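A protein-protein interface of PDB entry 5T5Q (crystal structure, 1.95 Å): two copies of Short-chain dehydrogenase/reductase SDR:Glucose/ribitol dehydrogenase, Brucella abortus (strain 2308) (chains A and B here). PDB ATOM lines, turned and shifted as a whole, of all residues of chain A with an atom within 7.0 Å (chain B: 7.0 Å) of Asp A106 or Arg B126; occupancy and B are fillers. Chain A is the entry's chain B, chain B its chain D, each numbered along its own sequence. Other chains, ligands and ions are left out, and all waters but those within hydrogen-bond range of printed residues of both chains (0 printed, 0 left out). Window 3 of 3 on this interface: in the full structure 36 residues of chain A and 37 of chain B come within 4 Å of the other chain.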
ATOM      1  N   PHE A 101      -9.955  -0.415  26.333  1.00  0.00           N
ATOM      2  CA  PHE A 101      -8.528  -0.177  26.122  1.00  0.00           C
ATOM      3  C   PHE A 101      -7.916   0.696  27.208  1.00  0.00           C
ATOM      4  O   PHE A 101      -6.745   0.521  27.566  1.00  0.00           O
ATOM      5  CB  PHE A 101      -8.283   0.452  24.748  1.00  0.00           C
ATOM      6  CG  PHE A 101      -6.830   0.489  24.369  1.00  0.00           C
ATOM      7  CD1 PHE A 101      -6.143  -0.687  24.119  1.00  0.00           C
ATOM      8  CD2 PHE A 101      -6.143   1.692  24.293  1.00  0.00           C
ATOM      9  CE1 PHE A 101      -4.803  -0.676  23.789  1.00  0.00           C
ATOM     10  CE2 PHE A 101      -4.801   1.716  23.955  1.00  0.00           C
ATOM     11  CZ  PHE A 101      -4.127   0.525  23.710  1.00  0.00           C
ATOM     12  N   GLU A 103      -8.531   0.600  30.248  1.00  0.00           N
ATOM     13  CA  GLU A 103      -8.382  -0.210  31.454  1.00  0.00           C
ATOM     14  C   GLU A 103      -7.472  -1.416  31.257  1.00  0.00           C
ATOM     15  O   GLU A 103      -7.304  -2.206  32.193  1.00  0.00           O
ATOM     16  CB  GLU A 103      -9.746  -0.719  31.933  1.00  0.00           C
ATOM     17  CG  GLU A 103     -10.811   0.333  32.179  1.00  0.00           C
ATOM     18  CD  GLU A 103     -12.200  -0.278  32.260  1.00  0.00           C
ATOM     19  OE1 GLU A 103     -12.302  -1.508  32.465  1.00  0.00           O
ATOM     20  OE2 GLU A 103     -13.192   0.465  32.126  1.00  0.00           O
ATOM     21  N   MET A 104      -6.904  -1.590  30.064  1.00  0.00           N
ATOM     22  CA  MET A 104      -6.191  -2.816  29.724  1.00  0.00           C
ATOM     23  C   MET A 104      -4.812  -2.820  30.373  1.00  0.00           C
ATOM     24  O   MET A 104      -3.987  -1.948  30.087  1.00  0.00           O
ATOM     25  CB  MET A 104      -6.070  -2.959  28.208  1.00  0.00           C
ATOM     26  CG  MET A 104      -5.396  -4.256  27.778  1.00  0.00           C
ATOM     27  SD  MET A 104      -5.435  -4.489  25.999  1.00  0.00           S
ATOM     28  CE  MET A 104      -7.175  -4.773  25.703  1.00  0.00           C
ATOM     29  N   SER A 105      -4.555  -3.808  31.229  1.00  0.00           N
ATOM     30  CA  SER A 105      -3.256  -3.924  31.875  1.00  0.00           C
ATOM     31  C   SER A 105      -2.245  -4.579  30.937  1.00  0.00           C
ATOM     32  O   SER A 105      -2.606  -5.267  29.977  1.00  0.00           O
ATOM     33  CB  SER A 105      -3.361  -4.752  33.150  1.00  0.00           C
ATOM     34  OG  SER A 105      -3.596  -6.111  32.830  1.00  0.00           O
ATOM     35  N   ASP A 106      -0.960  -4.385  31.243  1.00  0.00           N
ATOM     36  CA  ASP A 106       0.068  -5.105  30.496  1.00  0.00           C
ATOM     37  C   ASP A 106      -0.152  -6.611  30.596  1.00  0.00           C
ATOM     38  O   ASP A 106       0.068  -7.346  29.625  1.00  0.00           O
ATOM     39  CB  ASP A 106       1.465  -4.731  30.996  1.00  0.00           C
ATOM     40  CG  ASP A 106       1.882  -3.325  30.600  1.00  0.00           C
ATOM     41  OD1 ASP A 106       1.126  -2.648  29.871  1.00  0.00           O
ATOM     42  OD2 ASP A 106       2.980  -2.894  31.017  1.00  0.00           O
ATOM     43  N   ALA A 107      -0.587  -7.086  31.765  1.00  0.00           N
ATOM     44  CA  ALA A 107      -0.892  -8.503  31.926  1.00  0.00           C
ATOM     45  C   ALA A 107      -2.061  -8.920  31.043  1.00  0.00           C
ATOM     46  O   ALA A 107      -2.024  -9.989  30.420  1.00  0.00           O
ATOM     47  CB  ALA A 107      -1.184  -8.811  33.396  1.00  0.00           C
ATOM     48  N   ASP A 108      -3.111  -8.091  30.975  1.00  0.00           N
ATOM     49  CA  ASP A 108      -4.213  -8.381  30.065  1.00  0.00           C
ATOM     50  C   ASP A 108      -3.692  -8.597  28.654  1.00  0.00           C
ATOM     51  O   ASP A 108      -4.048  -9.575  27.986  1.00  0.00           O
ATOM     52  CB  ASP A 108      -5.239  -7.242  30.052  1.00  0.00           C
ATOM     53  CG  ASP A 108      -6.059  -7.158  31.317  1.00  0.00           C
ATOM     54  OD1 ASP A 108      -6.317  -8.210  31.932  1.00  0.00           O
ATOM     55  OD2 ASP A 108      -6.503  -6.034  31.652  1.00  0.00           O
ATOM     56  N   TRP A 109      -2.834  -7.686  28.189  1.00  0.00           N
ATOM     57  CA  TRP A 109      -2.364  -7.754  26.812  1.00  0.00           C
ATOM     58  C   TRP A 109      -1.582  -9.036  26.568  1.00  0.00           C
ATOM     59  O   TRP A 109      -1.893  -9.801  25.644  1.00  0.00           O
ATOM     60  CB  TRP A 109      -1.509  -6.533  26.478  1.00  0.00           C
ATOM     61  CG  TRP A 109      -0.864  -6.632  25.130  1.00  0.00           C
ATOM     62  CD1 TRP A 109       0.359  -7.169  24.841  1.00  0.00           C
ATOM     63  CD2 TRP A 109      -1.405  -6.170  23.882  1.00  0.00           C
ATOM     64  NE1 TRP A 109       0.606  -7.084  23.491  1.00  0.00           N
ATOM     65  CE2 TRP A 109      -0.459  -6.475  22.879  1.00  0.00           C
ATOM     66  CE3 TRP A 109      -2.600  -5.543  23.517  1.00  0.00           C
ATOM     67  CZ2 TRP A 109      -0.671  -6.171  21.526  1.00  0.00           C
ATOM     68  CZ3 TRP A 109      -2.808  -5.225  22.175  1.00  0.00           C
ATOM     69  CH2 TRP A 109      -1.845  -5.545  21.196  1.00  0.00           C
ATOM     70  N   HIS A 110      -0.575  -9.297  27.410  1.00  0.00           N
ATOM     71  CA  HIS A 110       0.308 -10.439  27.192  1.00  0.00           C
ATOM     72  C   HIS A 110      -0.445 -11.760  27.250  1.00  0.00           C
ATOM     73  O   HIS A 110      -0.154 -12.679  26.476  1.00  0.00           O
ATOM     74  CB  HIS A 110       1.438 -10.445  28.217  1.00  0.00           C
ATOM     75  CG  HIS A 110       2.460  -9.381  27.994  1.00  0.00           C
ATOM     76  ND1 HIS A 110       3.106  -9.215  26.787  1.00  0.00           N
ATOM     77  CD2 HIS A 110       2.971  -8.443  28.828  1.00  0.00           C
ATOM     78  CE1 HIS A 110       3.952  -8.206  26.878  1.00  0.00           C
ATOM     79  NE2 HIS A 110       3.893  -7.722  28.107  1.00  0.00           N
ATOM     80  N   ARG A 111      -1.405 -11.887  28.167  1.00  0.00           N
ATOM     81  CA  ARG A 111      -2.122 -13.154  28.269  1.00  0.00           C
ATOM     82  C   ARG A 111      -2.873 -13.473  26.979  1.00  0.00           C
ATOM     83  O   ARG A 111      -2.884 -14.627  26.528  1.00  0.00           O
ATOM     84  CB  ARG A 111      -3.076 -13.130  29.459  1.00  0.00           C
ATOM     85  CG  ARG A 111      -3.649 -14.484  29.745  1.00  0.00           C
ATOM     86  CD  ARG A 111      -4.278 -14.566  31.117  1.00  0.00           C
ATOM     87  NE  ARG A 111      -5.525 -15.327  31.069  1.00  0.00           N
ATOM     88  CZ  ARG A 111      -5.594 -16.655  31.068  1.00  0.00           C
ATOM     89  NH1 ARG A 111      -6.777 -17.254  31.015  1.00  0.00           N
ATOM     90  NH2 ARG A 111      -4.484 -17.383  31.111  1.00  0.00           N
ATOM     91  N   ALA B  69       8.038  -1.456  28.214  1.00  0.00           N
ATOM     92  CA  ALA B  69       6.844  -0.741  28.656  1.00  0.00           C
ATOM     93  C   ALA B  69       7.213   0.531  29.397  1.00  0.00           C
ATOM     94  O   ALA B  69       6.540   1.558  29.260  1.00  0.00           O
ATOM     95  CB  ALA B  69       5.992  -1.643  29.551  1.00  0.00           C
ATOM     96  N   ASP B  70       8.283   0.478  30.190  1.00  0.00           N
ATOM     97  CA  ASP B  70       8.690   1.652  30.950  1.00  0.00           C
ATOM     98  C   ASP B  70       9.164   2.774  30.030  1.00  0.00           C
ATOM     99  O   ASP B  70       8.944   3.952  30.335  1.00  0.00           O
ATOM    100  CB  ASP B  70       9.771   1.264  31.972  1.00  0.00           C
ATOM    101  CG  ASP B  70       9.251   0.298  33.061  1.00  0.00           C
ATOM    102  OD1 ASP B  70       8.045  -0.028  33.079  1.00  0.00           O
ATOM    103  OD2 ASP B  70      10.058  -0.145  33.908  1.00  0.00           O
ATOM    104  N   ASP B  71       9.775   2.437  28.884  1.00  0.00           N
ATOM    105  CA  ASP B  71      10.183   3.475  27.933  1.00  0.00           C
ATOM    106  C   ASP B  71       8.989   4.145  27.272  1.00  0.00           C
ATOM    107  O   ASP B  71       9.061   5.330  26.929  1.00  0.00           O
ATOM    108  CB  ASP B  71      11.094   2.909  26.847  1.00  0.00           C
ATOM    109  CG  ASP B  71      12.466   2.556  27.370  1.00  0.00           C
ATOM    110  OD1 ASP B  71      12.746   2.865  28.547  1.00  0.00           O
ATOM    111  OD2 ASP B  71      13.275   2.007  26.589  1.00  0.00           O
ATOM    112  N   ALA B  72       7.900   3.406  27.056  1.00  0.00           N
ATOM    113  CA  ALA B  72       6.675   4.043  26.582  1.00  0.00           C
ATOM    114  C   ALA B  72       6.191   5.094  27.582  1.00  0.00           C
ATOM    115  O   ALA B  72       5.777   6.194  27.193  1.00  0.00           O
ATOM    116  CB  ALA B  72       5.601   2.987  26.320  1.00  0.00           C
ATOM    117  N   GLU B  73       6.243   4.767  28.880  1.00  0.00           N
ATOM    118  CA  GLU B  73       5.890   5.725  29.925  1.00  0.00           C
ATOM    119  C   GLU B  73       6.805   6.946  29.901  1.00  0.00           C
ATOM    120  O   GLU B  73       6.340   8.089  30.039  1.00  0.00           O
ATOM    121  CB  GLU B  73       5.951   5.033  31.285  1.00  0.00           C
ATOM    122  CG  GLU B  73       4.960   3.889  31.403  1.00  0.00           C
ATOM    123  CD  GLU B  73       4.843   3.335  32.808  1.00  0.00           C
ATOM    124  OE1 GLU B  73       5.689   3.671  33.668  1.00  0.00           O
ATOM    125  OE2 GLU B  73       3.893   2.557  33.046  1.00  0.00           O
ATOM    126  N   LYS B  74       8.113   6.728  29.746  1.00  0.00           N
ATOM    127  CA  LYS B  74       9.032   7.858  29.685  1.00  0.00           C
ATOM    128  C   LYS B  74       8.740   8.729  28.476  1.00  0.00           C
ATOM    129  O   LYS B  74       8.740   9.964  28.566  1.00  0.00           O
ATOM    130  CB  LYS B  74      10.479   7.362  29.650  1.00  0.00           C
ATOM    131  N   VAL B  76       5.870   9.233  26.856  1.00  0.00           N
ATOM    132  CA  VAL B  76       4.677  10.051  27.055  1.00  0.00           C
ATOM    133  C   VAL B  76       4.947  11.168  28.063  1.00  0.00           C
ATOM    134  O   VAL B  76       4.544  12.321  27.857  1.00  0.00           O
ATOM    135  CB  VAL B  76       3.497   9.165  27.489  1.00  0.00           C
ATOM    136  CG1 VAL B  76       2.279  10.009  27.823  1.00  0.00           C
ATOM    137  CG2 VAL B  76       3.169   8.133  26.403  1.00  0.00           C
ATOM    138  N   ALA B  77       5.646  10.853  29.157  1.00  0.00           N
ATOM    139  CA  ALA B  77       5.947  11.878  30.152  1.00  0.00           C
ATOM    140  C   ALA B  77       6.757  13.015  29.536  1.00  0.00           C
ATOM    141  O   ALA B  77       6.459  14.196  29.759  1.00  0.00           O
ATOM    142  CB  ALA B  77       6.689  11.252  31.329  1.00  0.00           C
ATOM    143  N   ILE B  86      -0.045  15.223  23.011  1.00  0.00           N
ATOM    144  CA  ILE B  86       0.254  14.486  21.795  1.00  0.00           C
ATOM    145  C   ILE B  86      -0.850  14.755  20.784  1.00  0.00           C
ATOM    146  O   ILE B  86      -2.037  14.608  21.101  1.00  0.00           O
ATOM    147  CB  ILE B  86       0.376  12.977  22.067  1.00  0.00           C
ATOM    148  CG1 ILE B  86       1.456  12.710  23.120  1.00  0.00           C
ATOM    149  CG2 ILE B  86       0.700  12.240  20.770  1.00  0.00           C
ATOM    150  CD1 ILE B  86       1.531  11.252  23.572  1.00  0.00           C
ATOM    151  N   VAL B 120       3.890  -1.574  20.206  1.00  0.00           N
ATOM    152  CA  VAL B 120       2.822  -0.698  19.746  1.00  0.00           C
ATOM    153  C   VAL B 120       1.732  -0.604  20.809  1.00  0.00           C
ATOM    154  O   VAL B 120       1.237   0.489  21.115  1.00  0.00           O
ATOM    155  CB  VAL B 120       2.290  -1.186  18.386  1.00  0.00           C
ATOM    156  CG1 VAL B 120       1.132  -0.331  17.925  1.00  0.00           C
ATOM    157  CG2 VAL B 120       3.419  -1.144  17.353  1.00  0.00           C
ATOM    158  N   PHE B 121       1.390  -1.733  21.438  1.00  0.00           N
ATOM    159  CA  PHE B 121       0.446  -1.685  22.549  1.00  0.00           C
ATOM    160  C   PHE B 121       0.924  -0.749  23.644  1.00  0.00           C
ATOM    161  O   PHE B 121       0.162   0.104  24.110  1.00  0.00           O
ATOM    162  CB  PHE B 121       0.195  -3.065  23.150  1.00  0.00           C
ATOM    163  CG  PHE B 121      -0.426  -2.992  24.519  1.00  0.00           C
ATOM    164  CD1 PHE B 121      -1.714  -2.510  24.677  1.00  0.00           C
ATOM    165  CD2 PHE B 121       0.282  -3.373  25.646  1.00  0.00           C
ATOM    166  CE1 PHE B 121      -2.290  -2.407  25.923  1.00  0.00           C
ATOM    167  CE2 PHE B 121      -0.291  -3.276  26.904  1.00  0.00           C
ATOM    168  CZ  PHE B 121      -1.580  -2.792  27.046  1.00  0.00           C
ATOM    169  N   TYR B 122       2.180  -0.908  24.081  1.00  0.00           N
ATOM    170  CA  TYR B 122       2.676  -0.114  25.200  1.00  0.00           C
ATOM    171  C   TYR B 122       2.538   1.373  24.907  1.00  0.00           C
ATOM    172  O   TYR B 122       2.041   2.144  25.740  1.00  0.00           O
ATOM    173  CB  TYR B 122       4.144  -0.447  25.497  1.00  0.00           C
ATOM    174  CG  TYR B 122       4.439  -1.854  25.986  1.00  0.00           C
ATOM    175  CD1 TYR B 122       3.542  -2.541  26.790  1.00  0.00           C
ATOM    176  CD2 TYR B 122       5.644  -2.468  25.678  1.00  0.00           C
ATOM    177  CE1 TYR B 122       3.827  -3.824  27.241  1.00  0.00           C
ATOM    178  CE2 TYR B 122       5.937  -3.746  26.121  1.00  0.00           C
ATOM    179  CZ  TYR B 122       5.027  -4.418  26.898  1.00  0.00           C
ATOM    180  OH  TYR B 122       5.327  -5.683  27.335  1.00  0.00           O
ATOM    181  N   LEU B 123       2.949   1.784  23.706  1.00  0.00           N
ATOM    182  CA  LEU B 123       2.939   3.196  23.350  1.00  0.00           C
ATOM    183  C   LEU B 123       1.512   3.725  23.244  1.00  0.00           C
ATOM    184  O   LEU B 123       1.195   4.794  23.777  1.00  0.00           O
ATOM    185  CB  LEU B 123       3.693   3.398  22.036  1.00  0.00           C
ATOM    186  CG  LEU B 123       4.018   4.842  21.664  1.00  0.00           C
ATOM    187  CD1 LEU B 123       5.086   5.389  22.596  1.00  0.00           C
ATOM    188  CD2 LEU B 123       4.449   4.963  20.206  1.00  0.00           C
ATOM    189  N   CYS B 124       0.628   2.983  22.569  1.00  0.00           N
ATOM    190  CA  CYS B 124      -0.757   3.432  22.463  1.00  0.00           C
ATOM    191  C   CYS B 124      -1.419   3.529  23.838  1.00  0.00           C
ATOM    192  O   CYS B 124      -2.112   4.506  24.133  1.00  0.00           O
ATOM    193  CB  CYS B 124      -1.547   2.496  21.546  1.00  0.00           C
ATOM    194  SG  CYS B 124      -1.057   2.593  19.795  1.00  0.00           S
ATOM    195  N   LYS B 125      -1.208   2.528  24.692  1.00  0.00           N
ATOM    196  CA  LYS B 125      -1.830   2.522  26.015  1.00  0.00           C
ATOM    197  C   LYS B 125      -1.326   3.666  26.884  1.00  0.00           C
ATOM    198  O   LYS B 125      -2.118   4.362  27.530  1.00  0.00           O
ATOM    199  CB  LYS B 125      -1.577   1.191  26.718  1.00  0.00           C
ATOM    200  CG  LYS B 125      -2.079   1.179  28.152  1.00  0.00           C
ATOM    201  CD  LYS B 125      -3.586   1.391  28.211  1.00  0.00           C
ATOM    202  CE  LYS B 125      -4.094   1.263  29.642  1.00  0.00           C
ATOM    203  NZ  LYS B 125      -3.301   2.136  30.540  1.00  0.00           N
ATOM    204  N   ARG B 126      -0.008   3.861  26.936  1.00  0.00           N
ATOM    205  CA  ARG B 126       0.521   4.929  27.776  1.00  0.00           C
ATOM    206  C   ARG B 126       0.167   6.314  27.246  1.00  0.00           C
ATOM    207  O   ARG B 126       0.129   7.272  28.028  1.00  0.00           O
ATOM    208  CB  ARG B 126       2.044   4.801  27.923  1.00  0.00           C
ATOM    209  CG  ARG B 126       2.542   3.487  28.536  1.00  0.00           C
ATOM    210  CD  ARG B 126       1.677   2.998  29.706  1.00  0.00           C
ATOM    211  NE  ARG B 126       2.369   2.009  30.540  1.00  0.00           N
ATOM    212  CZ  ARG B 126       2.325   0.688  30.373  1.00  0.00           C
ATOM    213  NH1 ARG B 126       1.625   0.150  29.386  1.00  0.00           N
ATOM    214  NH2 ARG B 126       2.997  -0.105  31.200  1.00  0.00           N
ATOM    215  N   ALA B 127      -0.117   6.441  25.948  1.00  0.00           N
ATOM    216  CA  ALA B 127      -0.361   7.746  25.349  1.00  0.00           C
ATOM    217  C   ALA B 127      -1.756   8.291  25.625  1.00  0.00           C
ATOM    218  O   ALA B 127      -1.963   9.502  25.471  1.00  0.00           O
ATOM    219  CB  ALA B 127      -0.146   7.677  23.832  1.00  0.00           C
ATOM    220  N   LEU B 128      -2.711   7.434  26.002  1.00  0.00           N
ATOM    221  CA  LEU B 128      -4.122   7.823  26.085  1.00  0.00           C
ATOM    222  C   LEU B 128      -4.400   9.122  26.844  1.00  0.00           C
ATOM    223  O   LEU B 128      -5.106   9.986  26.295  1.00  0.00           O
ATOM    224  CB  LEU B 128      -4.924   6.663  26.687  1.00  0.00           C
ATOM    225  CG  LEU B 128      -4.999   5.404  25.836  1.00  0.00           C
ATOM    226  CD1 LEU B 128      -5.908   4.422  26.534  1.00  0.00           C
ATOM    227  CD2 LEU B 128      -5.521   5.729  24.446  1.00  0.00           C
ATOM    228  N   PRO B 129      -3.911   9.329  28.077  1.00  0.00           N
ATOM    229  CA  PRO B 129      -4.230  10.587  28.784  1.00  0.00           C
ATOM    230  C   PRO B 129      -3.647  11.821  28.123  1.00  0.00           C
ATOM    231  O   PRO B 129      -4.153  12.930  28.359  1.00  0.00           O
ATOM    232  CB  PRO B 129      -3.627  10.380  30.182  1.00  0.00           C
ATOM    233  CG  PRO B 129      -3.398   8.937  30.307  1.00  0.00           C
ATOM    234  CD  PRO B 129      -3.099   8.435  28.919  1.00  0.00           C
ATOM    235  N   ALA B 130      -2.607  11.664  27.306  1.00  0.00           N
ATOM    236  CA  ALA B 130      -1.915  12.778  26.678  1.00  0.00           C
ATOM    237  C   ALA B 130      -2.484  13.141  25.309  1.00  0.00           C
ATOM    238  O   ALA B 130      -2.111  14.180  24.754  1.00  0.00           O
ATOM    239  CB  ALA B 130      -0.418  12.456  26.553  1.00  0.00           C
ATOM    240  N   LEU B 131      -3.390  12.332  24.755  1.00  0.00           N
ATOM    241  CA  LEU B 131      -3.922  12.623  23.428  1.00  0.00           C
ATOM    242  C   LEU B 131      -4.808  13.867  23.474  1.00  0.00           C
ATOM    243  O   LEU B 131      -5.659  14.009  24.359  1.00  0.00           O
ATOM    244  CB  LEU B 131      -4.706  11.423  22.893  1.00  0.00           C
ATOM    245  CG  LEU B 131      -3.840  10.202  22.570  1.00  0.00           C
ATOM    246  CD1 LEU B 131      -4.705   8.996  22.250  1.00  0.00           C
ATOM    247  CD2 LEU B 131      -2.876  10.498  21.430  1.00  0.00           C
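Hydrophobic or aromatic side chains of chain A within 4 Å of the printed part of chain B: Phe A101, Met A104, Trp A109 and His A110.
Among the printed residues, 13 pairs touch across the chains.
Among the printed residues, Asp or Glu carboxylates within 4 Å of a Lys or Arg side-chain nitrogen of the other chain: Asp A106 with Arg B126 (2.8 Å).
A ring nitrogen (NE2) of His A110 lies within hydrogen-bond range of the side-chain hydroxyl (OH) of Tyr B122, 2.6 Å away.
The guanidinium group of Arg B126 lies within salt-bridge range of the side-chain carboxylate of Asp A106 (2.8 Å).
The backbone carbonyl oxygen of Val B120 lies within hydrogen-bond range of the side-chain sulfur of Cys B124, at 3.4 Å.
The side-chain hydroxyl (OG) of Ser A105 sits close to the backbone NH (N) of Ala A107, 3.3 Å away.
OE2 of Glu B73 is in salt-bridge range of NE of Arg B126 (3.0 Å).
OG of Ser A105 sits at hydrogen-bond distance from N of Asp A108, at 2.8 Å.
No position is printed for both chains.
Among the printed residues, pairs that only touch across the chains: Phe A101 with Phe B121 (3.7 Å), Phe A101 with Cys B124 (3.8 Å), Phe A101 with Lys B125 (3.3 Å), Phe A101 with Leu B128 (3.5 Å), Met A104 with Phe B121 (3.8 Å), Met A104 with Lys B125 (3.2 Å), Ser A105 with Phe B121 (3.97 Å), Asp A106 with Ala B69 (3.6 Å), Asp A106 with Phe B121 (3.3 Å), Asp A106 with Tyr B122 (3.9 Å) and Trp A109 with Phe B121 (3.4 Å).
Asp A106 touches just these residues of chain B: Ala B69, Phe B121, Tyr B122 and Arg B126.
Arg B126 touches just one residue of chain A: Asp A106.
Printed residues of chain B within 4 Å of Trp A109: Phe B121.
Of the printed residues of chain A, Ala B69 touches Asp A106 (3.6 Å).
Arg A111 touches none of the printed residues of chain B.
The nearest printed residue of chain A that does not touch Arg B126 is Met A104 (6.0 Å).
The nearest printed residue of chain A that does not touch Phe B121 is His A110 (6.0 Å).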
